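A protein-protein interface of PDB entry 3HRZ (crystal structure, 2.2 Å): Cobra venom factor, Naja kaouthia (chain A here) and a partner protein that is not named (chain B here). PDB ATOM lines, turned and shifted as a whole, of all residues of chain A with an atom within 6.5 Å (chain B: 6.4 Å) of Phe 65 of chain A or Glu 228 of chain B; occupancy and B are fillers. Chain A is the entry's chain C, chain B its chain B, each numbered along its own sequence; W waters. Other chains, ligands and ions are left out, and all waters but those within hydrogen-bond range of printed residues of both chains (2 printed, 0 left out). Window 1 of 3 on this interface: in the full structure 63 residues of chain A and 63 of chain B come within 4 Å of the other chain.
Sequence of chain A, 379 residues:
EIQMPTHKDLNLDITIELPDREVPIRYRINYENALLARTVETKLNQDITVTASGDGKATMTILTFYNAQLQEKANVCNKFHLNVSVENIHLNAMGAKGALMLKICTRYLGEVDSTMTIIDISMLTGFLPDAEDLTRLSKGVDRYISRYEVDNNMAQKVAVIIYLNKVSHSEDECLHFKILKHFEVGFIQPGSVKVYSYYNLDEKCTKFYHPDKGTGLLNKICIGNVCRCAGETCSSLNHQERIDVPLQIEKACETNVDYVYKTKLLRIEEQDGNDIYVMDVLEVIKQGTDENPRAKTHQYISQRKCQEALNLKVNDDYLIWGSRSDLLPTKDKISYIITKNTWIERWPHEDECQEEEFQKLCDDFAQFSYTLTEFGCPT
Printed residues of chain B that touch a printed residue of chain A: Gln 189, Lys 190, Ser 191, Ile 192, Leu 218, Ile 227, Glu 228, Thr 229 and Lys 230. Printed residues of chain A that touch a printed residue of chain B: Glu 41, Thr 42, Lys 43, Leu 44, Leu 63, Thr 64, Phe 65, Tyr 66 and Asn 67. Among the printed residues, 25 pairs touch across the chains. Among the printed residues, Asp or Glu carboxylates within 4 Å of a Lys or Arg side-chain nitrogen of the other chain: Glu 41 of chain A with Lys 230 of chain B (3.2 Å).
O of Ile 192 of chain B touches CA of Leu 63 of chain A (3.5 Å). O of Leu 63 of chain A touches CA of Thr 229 of chain B (3.2 Å). O of Thr 64 of chain A touches CA of Ser 191 of chain B, at 3.2 Å. CA of Thr 64 of chain A touches O of Glu 228 of chain B (3.7 Å). Thr 229 of chain B touches Thr 64 of chain A (OG1 to OG1, 3.8 Å). CA of Phe 65 of chain A touches O of Lys 190 of chain B (3.4 Å). Phe 65 of chain A touches Ile 227 of chain B (O to CA, 3.4 Å). Leu 218 of chain B touches Tyr 66 of chain A (CD2 to CD2, 3.3 Å). Tyr 66 of chain A touches Ile 227 of chain B (CB to CG1, 3.6 Å). ND2 of Asn 67 of chain A touches NE2 of Gln 189 of chain B (3.7 Å).
Water W1 lies within hydrogen-bond range of O of Lys 43 of chain A (2.6 Å) and N of Ile 227 of chain B (3.0 Å). Water W2 lies within hydrogen-bond range of OG1 of Thr 64 of chain A (2.7 Å) and O of Ile 192 of chain B (3.1 Å).
Of the printed residues of chain B, Leu 44 of chain A touches Thr 229. Printed residues of chain B within 4 Å of Phe 65 of chain A: Lys 190, Ser 191, Ile 227 and Glu 228. Printed residues of chain B within 4 Å of Tyr 66 of chain A: Gln 189, Lys 190, Leu 218 and Ile 227. Of the printed residues of chain A, Gln 189 of chain B touches Tyr 66 and Asn 67. Of chain A, only Glu 41 (3.5 Å), Thr 42 (3.7 Å), Leu 63 (3.6 Å), Thr 64 (3.7 Å) and Phe 65 (2.8 Å) come within 4 Å of Glu 228 of chain B. The nearest residue of chain A that does not touch Glu 228 of chain B is Lys 43 of chain A (4.5 Å).
The side-chain carboxylate (OE2) of Glu 228 of chain B is in salt-bridge range of the side-chain amino group (NZ) of Lys 230 of chain B, 3.2 Å away. The side-chain hydroxyl (OG1) of Thr 42 of chain A sits close to the backbone NH (N) of Leu 44 of chain A (3.5 Å).
O of Tyr 66 of chain A sits at hydrogen-bond distance from N of Lys 190 of chain B (3.0 Å). N of Ile 192 of chain B sits at hydrogen-bond distance from O of Thr 64 of chain A (2.8 Å). The backbone NH of Phe 65 of chain A sits at hydrogen-bond distance from the backbone carbonyl oxygen of Glu 228 of chain B, 2.8 Å away. The backbone carbonyl oxygen (O) of Thr 42 of chain A sits at hydrogen-bond distance from the backbone NH (N) of Thr 229 of chain B (3.0 Å). OG1 of Thr 229 of chain B sits at hydrogen-bond distance from O of Leu 44 of chain A. The side-chain carboxylate (OE2) of Glu 41 of chain A is in salt-bridge range of the side-chain amino group (NZ) of Lys 230 of chain B, at 3.2 Å. The backbone NH (N) of Lys 230 of chain B lies within hydrogen-bond range of the backbone carbonyl oxygen (O) of Leu 63 of chain A, 2.8 Å away. OE2 of Glu 41 of chain A lies close to OE2 of Glu 228 of chain B (3.5 Å). The backbone carbonyl oxygen of Lys 43 of chain A sits close to the backbone carbonyl oxygen of Ile 227 of chain B.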
ATOM      1  N   GLU A  41      21.128 -19.854 -15.318  1.00  0.00           N
ATOM      2  CA  GLU A  41      20.388 -20.635 -16.301  1.00  0.00           C
ATOM      3  C   GLU A  41      20.044 -22.025 -15.756  1.00  0.00           C
ATOM      4  O   GLU A  41      20.867 -22.668 -15.088  1.00  0.00           O
ATOM      5  CB  GLU A  41      21.196 -20.775 -17.594  1.00  0.00           C
ATOM      6  CG  GLU A  41      21.670 -19.452 -18.190  1.00  0.00           C
ATOM      7  CD  GLU A  41      22.989 -19.576 -18.948  1.00  0.00           C
ATOM      8  OE1 GLU A  41      24.016 -19.914 -18.311  1.00  0.00           O
ATOM      9  OE2 GLU A  41      23.004 -19.320 -20.176  1.00  0.00           O
ATOM     10  N   THR A  42      18.828 -22.477 -16.051  1.00  0.00           N
ATOM     11  CA  THR A  42      18.400 -23.827 -15.709  1.00  0.00           C
ATOM     12  C   THR A  42      17.653 -24.434 -16.891  1.00  0.00           C
ATOM     13  O   THR A  42      16.947 -23.734 -17.612  1.00  0.00           O
ATOM     14  CB  THR A  42      17.545 -23.862 -14.395  1.00  0.00           C
ATOM     15  OG1 THR A  42      17.240 -25.219 -14.042  1.00  0.00           O
ATOM     16  CG2 THR A  42      16.257 -23.074 -14.545  1.00  0.00           C
ATOM     17  N   LYS A  43      17.840 -25.729 -17.111  1.00  0.00           N
ATOM     18  CA  LYS A  43      17.206 -26.405 -18.234  1.00  0.00           C
ATOM     19  C   LYS A  43      15.848 -26.949 -17.823  1.00  0.00           C
ATOM     20  O   LYS A  43      15.226 -27.733 -18.545  1.00  0.00           O
ATOM     21  CB  LYS A  43      18.082 -27.546 -18.731  1.00  0.00           C
ATOM     22  CG  LYS A  43      19.338 -27.122 -19.453  1.00  0.00           C
ATOM     23  CD  LYS A  43      19.917 -28.299 -20.235  1.00  0.00           C
ATOM     24  CE  LYS A  43      21.080 -27.874 -21.116  1.00  0.00           C
ATOM     25  NZ  LYS A  43      20.693 -26.805 -22.081  1.00  0.00           N
ATOM     26  N   LEU A  44      15.386 -26.553 -16.651  1.00  0.00           N
ATOM     27  CA  LEU A  44      14.101 -27.031 -16.192  1.00  0.00           C
ATOM     28  C   LEU A  44      13.081 -25.911 -16.227  1.00  0.00           C
ATOM     29  O   LEU A  44      13.419 -24.735 -16.405  1.00  0.00           O
ATOM     30  CB  LEU A  44      14.220 -27.582 -14.777  1.00  0.00           C
ATOM     31  CG  LEU A  44      15.209 -28.736 -14.625  1.00  0.00           C
ATOM     32  CD1 LEU A  44      15.636 -28.883 -13.179  1.00  0.00           C
ATOM     33  CD2 LEU A  44      14.597 -30.031 -15.141  1.00  0.00           C
ATOM     34  N   LEU A  63      13.267 -15.243 -18.273  1.00  0.00           N
ATOM     35  CA  LEU A  63      13.009 -15.561 -19.665  1.00  0.00           C
ATOM     36  C   LEU A  63      12.866 -17.055 -19.801  1.00  0.00           C
ATOM     37  O   LEU A  63      13.807 -17.794 -19.517  1.00  0.00           O
ATOM     38  CB  LEU A  63      14.182 -15.111 -20.523  1.00  0.00           C
ATOM     39  CG  LEU A  63      14.511 -13.622 -20.478  1.00  0.00           C
ATOM     40  CD1 LEU A  63      15.715 -13.319 -21.376  1.00  0.00           C
ATOM     41  CD2 LEU A  63      13.287 -12.839 -20.913  1.00  0.00           C
ATOM     42  N   THR A  64      11.698 -17.514 -20.232  1.00  0.00           N
ATOM     43  CA  THR A  64      11.536 -18.937 -20.507  1.00  0.00           C
ATOM     44  C   THR A  64      11.452 -19.181 -22.002  1.00  0.00           C
ATOM     45  O   THR A  64      10.504 -18.752 -22.661  1.00  0.00           O
ATOM     46  CB  THR A  64      10.305 -19.542 -19.801  1.00  0.00           C
ATOM     47  OG1 THR A  64      10.407 -19.312 -18.396  1.00  0.00           O
ATOM     48  CG2 THR A  64      10.253 -21.036 -20.031  1.00  0.00           C
ATOM     49  N   PHE A  65      12.456 -19.871 -22.531  1.00  0.00           N
ATOM     50  CA  PHE A  65      12.500 -20.217 -23.947  1.00  0.00           C
ATOM     51  C   PHE A  65      12.005 -21.632 -24.154  1.00  0.00           C
ATOM     52  O   PHE A  65      12.340 -22.534 -23.386  1.00  0.00           O
ATOM     53  CB  PHE A  65      13.927 -20.114 -24.481  1.00  0.00           C
ATOM     54  CG  PHE A  65      14.491 -18.728 -24.439  1.00  0.00           C
ATOM     55  CD1 PHE A  65      14.226 -17.828 -25.457  1.00  0.00           C
ATOM     56  CD2 PHE A  65      15.288 -18.320 -23.380  1.00  0.00           C
ATOM     57  CE1 PHE A  65      14.746 -16.542 -25.414  1.00  0.00           C
ATOM     58  CE2 PHE A  65      15.812 -17.036 -23.333  1.00  0.00           C
ATOM     59  CZ  PHE A  65      15.538 -16.147 -24.345  1.00  0.00           C
ATOM     60  N   TYR A  66      11.207 -21.830 -25.195  1.00  0.00           N
ATOM     61  CA  TYR A  66      10.724 -23.157 -25.527  1.00  0.00           C
ATOM     62  C   TYR A  66      10.244 -23.167 -26.968  1.00  0.00           C
ATOM     63  O   TYR A  66      10.022 -22.114 -27.558  1.00  0.00           O
ATOM     64  CB  TYR A  66       9.588 -23.563 -24.584  1.00  0.00           C
ATOM     65  CG  TYR A  66       8.272 -22.853 -24.835  1.00  0.00           C
ATOM     66  CD1 TYR A  66       7.184 -23.534 -25.373  1.00  0.00           C
ATOM     67  CD2 TYR A  66       8.114 -21.504 -24.528  1.00  0.00           C
ATOM     68  CE1 TYR A  66       5.971 -22.889 -25.605  1.00  0.00           C
ATOM     69  CE2 TYR A  66       6.904 -20.851 -24.749  1.00  0.00           C
ATOM     70  CZ  TYR A  66       5.840 -21.549 -25.288  1.00  0.00           C
ATOM     71  OH  TYR A  66       4.644 -20.906 -25.513  1.00  0.00           O
ATOM     72  N   ASN A  67      10.083 -24.354 -27.541  1.00  0.00           N
ATOM     73  CA  ASN A  67       9.521 -24.438 -28.880  1.00  0.00           C
ATOM     74  C   ASN A  67       8.011 -24.650 -28.868  1.00  0.00           C
ATOM     75  O   ASN A  67       7.502 -25.578 -28.237  1.00  0.00           O
ATOM     76  CB  ASN A  67      10.230 -25.503 -29.710  1.00  0.00           C
ATOM     77  CG  ASN A  67      11.419 -24.947 -30.463  1.00  0.00           C
ATOM     78  OD1 ASN A  67      11.424 -24.910 -31.695  1.00  0.00           O
ATOM     79  ND2 ASN A  67      12.426 -24.496 -29.732  1.00  0.00           N
ATOM     80  N   GLN B 189      10.541 -20.789 -31.887  1.00  0.00           N
ATOM     81  CA  GLN B 189      11.042 -20.506 -30.556  1.00  0.00           C
ATOM     82  C   GLN B 189      10.379 -19.259 -29.978  1.00  0.00           C
ATOM     83  O   GLN B 189      10.486 -18.166 -30.530  1.00  0.00           O
ATOM     84  CB  GLN B 189      12.564 -20.397 -30.538  1.00  0.00           C
ATOM     85  CG  GLN B 189      13.114 -20.251 -29.129  1.00  0.00           C
ATOM     86  CD  GLN B 189      14.444 -20.943 -28.942  1.00  0.00           C
ATOM     87  OE1 GLN B 189      15.420 -20.623 -29.616  1.00  0.00           O
ATOM     88  NE2 GLN B 189      14.490 -21.899 -28.017  1.00  0.00           N
ATOM     89  N   LYS B 190       9.671 -19.449 -28.872  1.00  0.00           N
ATOM     90  CA  LYS B 190       9.018 -18.356 -28.175  1.00  0.00           C
ATOM     91  C   LYS B 190       9.704 -18.103 -26.845  1.00  0.00           C
ATOM     92  O   LYS B 190      10.482 -18.927 -26.354  1.00  0.00           O
ATOM     93  CB  LYS B 190       7.545 -18.677 -27.928  1.00  0.00           C
ATOM     94  CG  LYS B 190       6.704 -18.735 -29.187  1.00  0.00           C
ATOM     95  CD  LYS B 190       5.245 -19.054 -28.877  1.00  0.00           C
ATOM     96  CE  LYS B 190       4.585 -17.932 -28.085  1.00  0.00           C
ATOM     97  NZ  LYS B 190       3.119 -18.163 -27.912  1.00  0.00           N
ATOM     98  N   SER B 191       9.410 -16.948 -26.267  1.00  0.00           N
ATOM     99  CA  SER B 191       9.894 -16.619 -24.942  1.00  0.00           C
ATOM    100  C   SER B 191       8.727 -16.131 -24.096  1.00  0.00           C
ATOM    101  O   SER B 191       7.908 -15.319 -24.540  1.00  0.00           O
ATOM    102  CB  SER B 191      10.980 -15.543 -25.012  1.00  0.00           C
ATOM    103  OG  SER B 191      10.440 -14.302 -25.434  1.00  0.00           O
ATOM    104  N   ILE B 192       8.638 -16.663 -22.885  1.00  0.00           N
ATOM    105  CA  ILE B 192       7.741 -16.115 -21.890  1.00  0.00           C
ATOM    106  C   ILE B 192       8.577 -15.211 -21.004  1.00  0.00           C
ATOM    107  O   ILE B 192       9.620 -15.621 -20.497  1.00  0.00           O
ATOM    108  CB  ILE B 192       7.102 -17.210 -21.046  1.00  0.00           C
ATOM    109  CG1 ILE B 192       6.097 -18.007 -21.886  1.00  0.00           C
ATOM    110  CG2 ILE B 192       6.425 -16.605 -19.821  1.00  0.00           C
ATOM    111  CD1 ILE B 192       5.493 -19.178 -21.150  1.00  0.00           C
ATOM    112  N   LEU B 218       3.121 -23.642 -20.160  1.00  0.00           N
ATOM    113  CA  LEU B 218       3.539 -23.839 -21.541  1.00  0.00           C
ATOM    114  C   LEU B 218       2.621 -24.816 -22.250  1.00  0.00           C
ATOM    115  O   LEU B 218       1.403 -24.627 -22.318  1.00  0.00           O
ATOM    116  CB  LEU B 218       4.960 -24.400 -21.579  1.00  0.00           C
ATOM    117  CG  LEU B 218       6.039 -23.542 -20.923  1.00  0.00           C
ATOM    118  CD1 LEU B 218       7.267 -24.365 -20.598  1.00  0.00           C
ATOM    119  CD2 LEU B 218       6.385 -22.395 -21.833  1.00  0.00           C
ATOM    120  N   GLU B 226      13.626 -29.031 -26.029  1.00  0.00           N
ATOM    121  CA  GLU B 226      14.273 -28.502 -24.839  1.00  0.00           C
ATOM    122  C   GLU B 226      13.686 -27.172 -24.365  1.00  0.00           C
ATOM    123  O   GLU B 226      13.039 -26.444 -25.122  1.00  0.00           O
ATOM    124  CB  GLU B 226      15.790 -28.402 -25.048  1.00  0.00           C
ATOM    125  CG  GLU B 226      16.540 -29.698 -24.750  1.00  0.00           C
ATOM    126  CD  GLU B 226      17.904 -29.765 -25.423  1.00  0.00           C
ATOM    127  OE1 GLU B 226      18.183 -28.915 -26.297  1.00  0.00           O
ATOM    128  OE2 GLU B 226      18.693 -30.676 -25.084  1.00  0.00           O
ATOM    129  N   ILE B 227      13.910 -26.878 -23.092  1.00  0.00           N
ATOM    130  CA  ILE B 227      13.433 -25.650 -22.481  1.00  0.00           C
ATOM    131  C   ILE B 227      14.547 -25.027 -21.656  1.00  0.00           C
ATOM    132  O   ILE B 227      15.197 -25.709 -20.864  1.00  0.00           O
ATOM    133  CB  ILE B 227      12.259 -25.929 -21.557  1.00  0.00           C
ATOM    134  CG1 ILE B 227      10.974 -26.059 -22.367  1.00  0.00           C
ATOM    135  CG2 ILE B 227      12.140 -24.841 -20.499  1.00  0.00           C
ATOM    136  CD1 ILE B 227       9.783 -26.398 -21.516  1.00  0.00           C
ATOM    137  N   GLU B 228      14.774 -23.735 -21.842  1.00  0.00           N
ATOM    138  CA  GLU B 228      15.787 -23.049 -21.058  1.00  0.00           C
ATOM    139  C   GLU B 228      15.215 -21.801 -20.409  1.00  0.00           C
ATOM    140  O   GLU B 228      14.589 -20.973 -21.070  1.00  0.00           O
ATOM    141  CB  GLU B 228      17.019 -22.702 -21.902  1.00  0.00           C
ATOM    142  CG  GLU B 228      18.210 -22.255 -21.045  1.00  0.00           C
ATOM    143  CD  GLU B 228      19.476 -21.992 -21.845  1.00  0.00           C
ATOM    144  OE1 GLU B 228      19.621 -22.555 -22.953  1.00  0.00           O
ATOM    145  OE2 GLU B 228      20.332 -21.224 -21.351  1.00  0.00           O
ATOM    146  N   THR B 229      15.419 -21.688 -19.103  1.00  0.00           N
ATOM    147  CA  THR B 229      15.041 -20.500 -18.354  1.00  0.00           C
ATOM    148  C   THR B 229      16.284 -19.674 -18.020  1.00  0.00           C
ATOM    149  O   THR B 229      17.273 -20.201 -17.503  1.00  0.00           O
ATOM    150  CB  THR B 229      14.341 -20.872 -17.031  1.00  0.00           C
ATOM    151  OG1 THR B 229      13.198 -21.694 -17.298  1.00  0.00           O
ATOM    152  CG2 THR B 229      13.911 -19.615 -16.286  1.00  0.00           C
ATOM    153  N   LYS B 230      16.241 -18.385 -18.330  1.00  0.00           N
ATOM    154  CA  LYS B 230      17.292 -17.470 -17.901  1.00  0.00           C
ATOM    155  C   LYS B 230      16.724 -16.568 -16.815  1.00  0.00           C
ATOM    156  O   LYS B 230      15.631 -16.008 -16.957  1.00  0.00           O
ATOM    157  CB  LYS B 230      17.836 -16.628 -19.067  1.00  0.00           C
ATOM    158  CG  LYS B 230      18.613 -17.417 -20.112  1.00  0.00           C
ATOM    159  CD  LYS B 230      19.340 -16.497 -21.083  1.00  0.00           C
ATOM    160  CE  LYS B 230      19.726 -17.222 -22.376  1.00  0.00           C
ATOM    161  NZ  LYS B 230      20.832 -18.222 -22.232  1.00  0.00           N
HETATM  162  O   HOH W   1      14.889 -28.770 -20.926  1.00  0.00           O
HETATM  163  O   HOH W   2       9.538 -16.893 -17.697  1.00  0.00           O
